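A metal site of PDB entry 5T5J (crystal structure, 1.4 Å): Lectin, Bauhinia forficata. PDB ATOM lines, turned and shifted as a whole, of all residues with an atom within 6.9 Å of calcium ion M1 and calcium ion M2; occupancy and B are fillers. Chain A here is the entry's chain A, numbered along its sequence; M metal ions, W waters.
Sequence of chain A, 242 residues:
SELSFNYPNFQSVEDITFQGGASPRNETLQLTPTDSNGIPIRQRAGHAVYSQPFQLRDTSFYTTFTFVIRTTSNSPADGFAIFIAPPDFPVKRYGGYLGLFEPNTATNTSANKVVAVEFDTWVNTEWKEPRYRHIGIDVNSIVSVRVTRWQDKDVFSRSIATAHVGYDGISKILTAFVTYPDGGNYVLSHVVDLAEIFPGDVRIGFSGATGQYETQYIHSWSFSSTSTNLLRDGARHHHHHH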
ATOM      1  N   ASP A  78     -19.924  15.068  17.550  1.00  0.00           N
ATOM      2  CA  ASP A  78     -20.891  14.989  16.410  1.00  0.00           C
ATOM      3  C   ASP A  78     -22.188  14.231  16.710  1.00  0.00           C
ATOM      4  O   ASP A  78     -23.128  14.382  15.931  1.00  0.00           O
ATOM      5  CB  ASP A  78     -20.169  14.234  15.273  1.00  0.00           C
ATOM      6  CG  ASP A  78     -19.347  15.243  14.480  1.00  0.00           C
ATOM      7  OD1 ASP A  78     -19.893  15.890  13.578  1.00  0.00           O
ATOM      8  OD2 ASP A  78     -18.122  15.360  14.805  1.00  0.00           O
ATOM      9  N   GLY A  95     -15.836  12.307  13.377  1.00  0.00           N
ATOM     10  CA  GLY A  95     -16.532  13.461  12.891  1.00  0.00           C
ATOM     11  C   GLY A  95     -17.940  13.115  12.458  1.00  0.00           C
ATOM     12  O   GLY A  95     -18.634  12.252  13.060  1.00  0.00           O
ATOM     13  N   GLY A  96     -18.408  13.791  11.405  1.00  0.00           N
ATOM     14  CA  GLY A  96     -19.794  13.695  11.000  1.00  0.00           C
ATOM     15  C   GLY A  96     -20.224  12.377  10.445  1.00  0.00           C
ATOM     16  O   GLY A  96     -21.435  12.123  10.329  1.00  0.00           O
ATOM     17  N   TYR A  97     -19.274  11.534  10.130  1.00  0.00           N
ATOM     18  CA  TYR A  97     -19.580  10.159   9.721  1.00  0.00           C
ATOM     19  C   TYR A  97     -20.022   9.303  10.862  1.00  0.00           C
ATOM     20  O   TYR A  97     -20.455   8.152  10.609  1.00  0.00           O
ATOM     21  CB  TYR A  97     -18.343   9.579   9.004  1.00  0.00           C
ATOM     22  CG  TYR A  97     -17.865  10.426   7.894  1.00  0.00           C
ATOM     23  CD1 TYR A  97     -18.513  10.383   6.662  1.00  0.00           C
ATOM     24  CD2 TYR A  97     -16.748  11.281   7.993  1.00  0.00           C
ATOM     25  CE1 TYR A  97     -18.125  11.225   5.629  1.00  0.00           C
ATOM     26  CE2 TYR A  97     -16.388  12.088   6.953  1.00  0.00           C
ATOM     27  CZ  TYR A  97     -17.028  12.088   5.767  1.00  0.00           C
ATOM     28  OH  TYR A  97     -16.623  12.894   4.731  1.00  0.00           O
ATOM     29  N   LEU A  98     -19.885   9.762  12.086  1.00  0.00           N
ATOM     30  CA  LEU A  98     -20.489   9.106  13.247  1.00  0.00           C
ATOM     31  C   LEU A  98     -19.935   7.748  13.558  1.00  0.00           C
ATOM     32  O   LEU A  98     -20.572   6.980  14.257  1.00  0.00           O
ATOM     33  CB  LEU A  98     -22.044   9.070  13.225  1.00  0.00           C
ATOM     34  CG  LEU A  98     -22.720  10.435  13.266  1.00  0.00           C
ATOM     35  CD1 LEU A  98     -24.221  10.304  13.107  1.00  0.00           C
ATOM     36  CD2 LEU A  98     -22.432  11.181  14.537  1.00  0.00           C
ATOM     37  N   GLU A 118     -29.788   7.844  14.459  1.00  0.00           N
ATOM     38  CA  GLU A 118     -28.730   8.809  14.827  1.00  0.00           C
ATOM     39  C   GLU A 118     -29.287   9.973  15.646  1.00  0.00           C
ATOM     40  O   GLU A 118     -30.445  10.406  15.442  1.00  0.00           O
ATOM     41  CB  GLU A 118     -27.991   9.358  13.596  1.00  0.00           C
ATOM     42  CG  GLU A 118     -28.894  10.142  12.655  1.00  0.00           C
ATOM     43  CD  GLU A 118     -28.071  10.963  11.641  1.00  0.00           C
ATOM     44  OE1 GLU A 118     -27.178  10.319  10.968  1.00  0.00           O
ATOM     45  OE2 GLU A 118     -28.237  12.181  11.541  1.00  0.00           O
ATOM     46  N   PHE A 119     -28.431  10.473  16.500  1.00  0.00           N
ATOM     47  CA  PHE A 119     -28.671  11.589  17.390  1.00  0.00           C
ATOM     48  C   PHE A 119     -27.556  12.602  17.019  1.00  0.00           C
ATOM     49  O   PHE A 119     -26.383  12.407  17.442  1.00  0.00           O
ATOM     50  CB  PHE A 119     -28.565  11.155  18.852  1.00  0.00           C
ATOM     51  CG  PHE A 119     -29.615  10.129  19.219  1.00  0.00           C
ATOM     52  CD1 PHE A 119     -29.462   8.798  18.841  1.00  0.00           C
ATOM     53  CD2 PHE A 119     -30.770  10.464  19.878  1.00  0.00           C
ATOM     54  CE1 PHE A 119     -30.423   7.865  19.131  1.00  0.00           C
ATOM     55  CE2 PHE A 119     -31.712   9.512  20.223  1.00  0.00           C
ATOM     56  CZ  PHE A 119     -31.550   8.228  19.753  1.00  0.00           C
ATOM     57  N   ASP A 120     -27.869  13.541  16.160  1.00  0.00           N
ATOM     58  CA  ASP A 120     -26.862  14.340  15.439  1.00  0.00           C
ATOM     59  C   ASP A 120     -26.769  15.743  16.014  1.00  0.00           C
ATOM     60  O   ASP A 120     -27.714  16.492  15.873  1.00  0.00           O
ATOM     61  CB  ASP A 120     -27.220  14.305  13.937  1.00  0.00           C
ATOM     62  CG  ASP A 120     -26.108  14.872  13.039  1.00  0.00           C
ATOM     63  OD1 ASP A 120     -25.291  15.629  13.599  1.00  0.00           O
ATOM     64  OD2 ASP A 120     -26.077  14.523  11.833  1.00  0.00           O
ATOM     65  N   THR A 121     -25.614  16.056  16.604  1.00  0.00           N
ATOM     66  CA  THR A 121     -25.406  17.334  17.303  1.00  0.00           C
ATOM     67  C   THR A 121     -24.756  18.401  16.447  1.00  0.00           C
ATOM     68  O   THR A 121     -24.648  19.545  16.916  1.00  0.00           O
ATOM     69  CB  THR A 121     -24.586  17.141  18.585  1.00  0.00           C
ATOM     70  OG1 THR A 121     -23.306  16.658  18.210  1.00  0.00           O
ATOM     71  CG2 THR A 121     -25.225  16.196  19.595  1.00  0.00           C
ATOM     72  N   TRP A 122     -24.330  18.105  15.222  1.00  0.00           N
ATOM     73  CA  TRP A 122     -23.545  19.020  14.414  1.00  0.00           C
ATOM     74  C   TRP A 122     -24.081  18.984  12.972  1.00  0.00           C
ATOM     75  O   TRP A 122     -24.088  17.944  12.280  1.00  0.00           O
ATOM     76  CB  TRP A 122     -22.063  18.645  14.437  1.00  0.00           C
ATOM     77  CG  TRP A 122     -21.228  19.497  13.500  1.00  0.00           C
ATOM     78  CD1 TRP A 122     -21.104  19.282  12.164  1.00  0.00           C
ATOM     79  CD2 TRP A 122     -20.435  20.644  13.816  1.00  0.00           C
ATOM     80  NE1 TRP A 122     -20.274  20.250  11.580  1.00  0.00           N
ATOM     81  CE2 TRP A 122     -19.877  21.085  12.596  1.00  0.00           C
ATOM     82  CE3 TRP A 122     -20.200  21.355  14.975  1.00  0.00           C
ATOM     83  CZ2 TRP A 122     -19.014  22.197  12.493  1.00  0.00           C
ATOM     84  CZ3 TRP A 122     -19.284  22.459  14.866  1.00  0.00           C
ATOM     85  CH2 TRP A 122     -18.714  22.826  13.663  1.00  0.00           C
ATOM     86  N   VAL A 123     -24.554  20.153  12.498  1.00  0.00           N
ATOM     87  CA  VAL A 123     -25.062  20.254  11.154  1.00  0.00           C
ATOM     88  C   VAL A 123     -23.864  20.260  10.174  1.00  0.00           C
ATOM     89  O   VAL A 123     -23.111  21.230  10.085  1.00  0.00           O
ATOM     90  CB  VAL A 123     -25.928  21.504  11.017  1.00  0.00           C
ATOM     91  CG1 VAL A 123     -26.393  21.761   9.532  1.00  0.00           C
ATOM     92  CG2 VAL A 123     -27.130  21.482  11.916  1.00  0.00           C
ATOM     93  N   ASN A 124     -23.725  19.208   9.398  1.00  0.00           N
ATOM     94  CA  ASN A 124     -22.633  19.081   8.468  1.00  0.00           C
ATOM     95  C   ASN A 124     -22.948  19.831   7.180  1.00  0.00           C
ATOM     96  O   ASN A 124     -24.052  19.725   6.649  1.00  0.00           O
ATOM     97  CB  ASN A 124     -22.362  17.621   8.161  1.00  0.00           C
ATOM     98  CG  ASN A 124     -21.571  17.021   9.286  1.00  0.00           C
ATOM     99  OD1 ASN A 124     -22.140  16.448  10.230  1.00  0.00           O
ATOM    100  ND2 ASN A 124     -20.258  17.131   9.226  1.00  0.00           N
ATOM    101  N   TRP A 127     -22.649  17.310   3.306  1.00  0.00           N
ATOM    102  CA  TRP A 127     -23.718  16.541   2.693  1.00  0.00           C
ATOM    103  C   TRP A 127     -25.042  17.169   3.188  1.00  0.00           C
ATOM    104  O   TRP A 127     -25.014  18.041   4.103  1.00  0.00           O
ATOM    105  CB  TRP A 127     -23.644  15.057   3.019  1.00  0.00           C
ATOM    106  CG  TRP A 127     -23.528  14.760   4.487  1.00  0.00           C
ATOM    107  CD1 TRP A 127     -24.527  14.710   5.403  1.00  0.00           C
ATOM    108  CD2 TRP A 127     -22.344  14.499   5.189  1.00  0.00           C
ATOM    109  NE1 TRP A 127     -24.025  14.439   6.658  1.00  0.00           N
ATOM    110  CE2 TRP A 127     -22.654  14.325   6.548  1.00  0.00           C
ATOM    111  CE3 TRP A 127     -21.015  14.386   4.774  1.00  0.00           C
ATOM    112  CZ2 TRP A 127     -21.700  14.041   7.504  1.00  0.00           C
ATOM    113  CZ3 TRP A 127     -20.048  14.118   5.738  1.00  0.00           C
ATOM    114  CH2 TRP A 127     -20.420  13.948   7.100  1.00  0.00           C
ATOM    115  N   LYS A 128     -26.175  16.735   2.585  1.00  0.00           N
ATOM    116  CA  LYS A 128     -27.447  17.302   2.940  1.00  0.00           C
ATOM    117  C   LYS A 128     -27.819  16.883   4.357  1.00  0.00           C
ATOM    118  O   LYS A 128     -27.941  15.710   4.645  1.00  0.00           O
ATOM    119  CB  LYS A 128     -28.524  16.770   1.929  1.00  0.00           C
ATOM    120  CG  LYS A 128     -29.962  17.179   2.201  1.00  0.00           C
ATOM    121  CD  LYS A 128     -30.929  16.499   1.188  1.00  0.00           C
ATOM    122  CE  LYS A 128     -31.760  15.401   1.847  1.00  0.00           C
ATOM    123  NZ  LYS A 128     -33.032  16.007   2.353  1.00  0.00           N
ATOM    124  N   GLU A 129     -28.025  17.883   5.228  1.00  0.00           N
ATOM    125  CA  GLU A 129     -28.558  17.797   6.558  1.00  0.00           C
ATOM    126  C   GLU A 129     -29.526  18.894   6.803  1.00  0.00           C
ATOM    127  O   GLU A 129     -29.317  19.955   6.266  1.00  0.00           O
ATOM    128  CB  GLU A 129     -27.371  18.036   7.682  1.00  0.00           C
ATOM    129  CG  GLU A 129     -26.296  17.063   7.580  1.00  0.00           C
ATOM    130  CD  GLU A 129     -25.989  16.310   8.864  1.00  0.00           C
ATOM    131  OE1 GLU A 129     -26.426  15.162   8.881  1.00  0.00           O
ATOM    132  OE2 GLU A 129     -25.373  16.882   9.766  1.00  0.00           O
ATOM    133  N   PRO A 130     -30.536  18.675   7.693  1.00  0.00           N
ATOM    134  CA  PRO A 130     -31.343  19.845   8.063  1.00  0.00           C
ATOM    135  C   PRO A 130     -30.498  20.838   8.812  1.00  0.00           C
ATOM    136  O   PRO A 130     -29.524  20.452   9.445  1.00  0.00           O
ATOM    137  CB  PRO A 130     -32.413  19.252   8.968  1.00  0.00           C
ATOM    138  CG  PRO A 130     -32.008  17.910   9.310  1.00  0.00           C
ATOM    139  CD  PRO A 130     -30.936  17.430   8.391  1.00  0.00           C
ATOM    140  N   HIS A 134     -30.689  17.151  15.031  1.00  0.00           N
ATOM    141  CA  HIS A 134     -31.754  16.293  14.548  1.00  0.00           C
ATOM    142  C   HIS A 134     -31.567  14.837  15.016  1.00  0.00           C
ATOM    143  O   HIS A 134     -30.417  14.418  15.254  1.00  0.00           O
ATOM    144  CB  HIS A 134     -31.876  16.394  13.016  1.00  0.00           C
ATOM    145  CG  HIS A 134     -30.609  16.152  12.277  1.00  0.00           C
ATOM    146  ND1 HIS A 134     -29.672  17.165  12.075  1.00  0.00           N
ATOM    147  CD2 HIS A 134     -30.088  15.072  11.673  1.00  0.00           C
ATOM    148  CE1 HIS A 134     -28.625  16.687  11.452  1.00  0.00           C
ATOM    149  NE2 HIS A 134     -28.870  15.427  11.168  1.00  0.00           N
ATOM    150  N   GLY A 136     -32.454  11.048  13.342  1.00  0.00           N
ATOM    151  CA  GLY A 136     -32.714  10.529  12.029  1.00  0.00           C
ATOM    152  C   GLY A 136     -32.642   9.018  11.958  1.00  0.00           C
ATOM    153  O   GLY A 136     -31.969   8.375  12.751  1.00  0.00           O
ATOM    154  N   ASP A 138     -31.088   6.334   9.333  1.00  0.00           N
ATOM    155  CA  ASP A 138     -30.117   6.187   8.271  1.00  0.00           C
ATOM    156  C   ASP A 138     -30.171   4.792   7.679  1.00  0.00           C
ATOM    157  O   ASP A 138     -30.119   3.808   8.430  1.00  0.00           O
ATOM    158  CB  ASP A 138     -28.721   6.404   8.829  1.00  0.00           C
ATOM    159  CG  ASP A 138     -28.506   7.755   9.387  1.00  0.00           C
ATOM    160  OD1 ASP A 138     -29.313   8.663   9.181  1.00  0.00           O
ATOM    161  OD2 ASP A 138     -27.497   7.922  10.184  1.00  0.00           O
ATOM    162  N   ILE A 142     -25.123   8.345   5.201  1.00  0.00           N
ATOM    163  CA  ILE A 142     -25.098   9.370   6.241  1.00  0.00           C
ATOM    164  C   ILE A 142     -26.163  10.430   6.076  1.00  0.00           C
ATOM    165  O   ILE A 142     -26.446  11.213   6.985  1.00  0.00           O
ATOM    166  CB  ILE A 142     -23.659   9.940   6.362  1.00  0.00           C
ATOM    167  CG1 ILE A 142     -23.433  10.676   7.676  1.00  0.00           C
ATOM    168  CG2 ILE A 142     -23.325  10.838   5.185  1.00  0.00           C
ATOM    169  CD1 ILE A 142     -23.662   9.922   9.011  1.00  0.00           C
ATOM    170  N   VAL A 143     -26.777  10.510   4.887  1.00  0.00           N
ATOM    171  CA  VAL A 143     -27.941  11.388   4.642  1.00  0.00           C
ATOM    172  C   VAL A 143     -29.185  10.653   5.063  1.00  0.00           C
ATOM    173  O   VAL A 143     -29.540   9.670   4.391  1.00  0.00           O
ATOM    174  CB  VAL A 143     -27.989  11.851   3.152  1.00  0.00           C
ATOM    175  CG1 VAL A 143     -29.332  12.639   2.869  1.00  0.00           C
ATOM    176  CG2 VAL A 143     -26.743  12.668   2.807  1.00  0.00           C
ATOM    177  N   SER A 144     -29.797  11.065   6.148  1.00  0.00           N
ATOM    178  CA  SER A 144     -30.924  10.339   6.697  1.00  0.00           C
ATOM    179  C   SER A 144     -32.126  10.254   5.727  1.00  0.00           C
ATOM    180  O   SER A 144     -32.382  11.226   5.025  1.00  0.00           O
ATOM    181  CB  SER A 144     -31.391  11.021   7.964  1.00  0.00           C
ATOM    182  OG  SER A 144     -30.414  11.100   8.945  1.00  0.00           O
ATOM    183  N   VAL A 147     -35.965  12.351   9.087  1.00  0.00           N
ATOM    184  CA  VAL A 147     -35.255  13.162  10.026  1.00  0.00           C
ATOM    185  C   VAL A 147     -36.257  14.051  10.737  1.00  0.00           C
ATOM    186  O   VAL A 147     -37.239  14.498  10.117  1.00  0.00           O
ATOM    187  CB  VAL A 147     -34.100  13.830   9.309  1.00  0.00           C
ATOM    188  CG1 VAL A 147     -34.587  14.930   8.370  1.00  0.00           C
ATOM    189  CG2 VAL A 147     -33.034  14.233  10.121  1.00  0.00           C
HETATM  190 CA    CA M   1     -27.412  13.838  10.276  1.00  0.00          CA
HETATM  191 CA    CA M   2     -24.037  15.803  11.445  1.00  0.00          CA
HETATM  192  O   HOH W   1     -25.966  12.228   9.537  1.00  0.00           O
HETATM  193  O   HOH W   2     -28.927  13.373   8.781  1.00  0.00           O
HETATM  194  O   HOH W   3     -23.659  13.684  10.377  1.00  0.00           O
HETATM  195  O   HOH W   4     -22.478  15.180  13.164  1.00  0.00           O
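Four residues have an atom within 4 Å of calcium ion M1: Glu 118, Asp 120, Glu 129 and His 134.
The nearest printed residue that does not touch calcium ion M1 is Ser 144 (4.3 Å).
Of the 23 residues printed, 4 come within 4 Å of calcium ion M2.
OE1 of Glu 129 binds calcium ion M1, 2.2 Å away.
Calcium ion M1 is bound by OD2 of Asp 120 (2.2 Å).
Water W2 is bound to calcium ion M1 (2.2 Å).
OE2 of Glu 118 is bound to calcium ion M1, at 2.2 Å.
Calcium ion M1 is bound by water W1, at 2.3 Å.
Calcium ion M1 is bound by NE2 of His 134.
The side-chain carboxylate (OD2) of Asp 138 sits close to the side-chain carboxylate (OE1) of Glu 118, at 2.5 Å.
The backbone NH of Glu 118 is in hydrogen-bond range of the backbone carbonyl oxygen of Gly 136 (2.8 Å).
NE1 of Trp 127 sits close to OE1 of Glu 129 (3.4 Å).
The backbone carbonyl oxygen (O) of Trp 122 binds calcium ion M2 (2.3 Å).
Calcium ion M2 is bound by OD1 of Asn 124 (2.3 Å).
Calcium ion M2 is bound by OE2 of Glu 129 (2.4 Å).
Calcium ion M2 is bound by water W4, 2.4 Å away.
Calcium ion M2 is bound by water W3, at 2.4 Å.
OD2 of Asp 120 is bound to calcium ion M2 (2.4 Å).
Calcium ion M2 is bound by OD1 of Asp 120, at 2.5 Å.
Water W1 lies within hydrogen-bond range of OE1 of Glu 118 (2.7 Å) and O of Ile 142 (2.8 Å).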
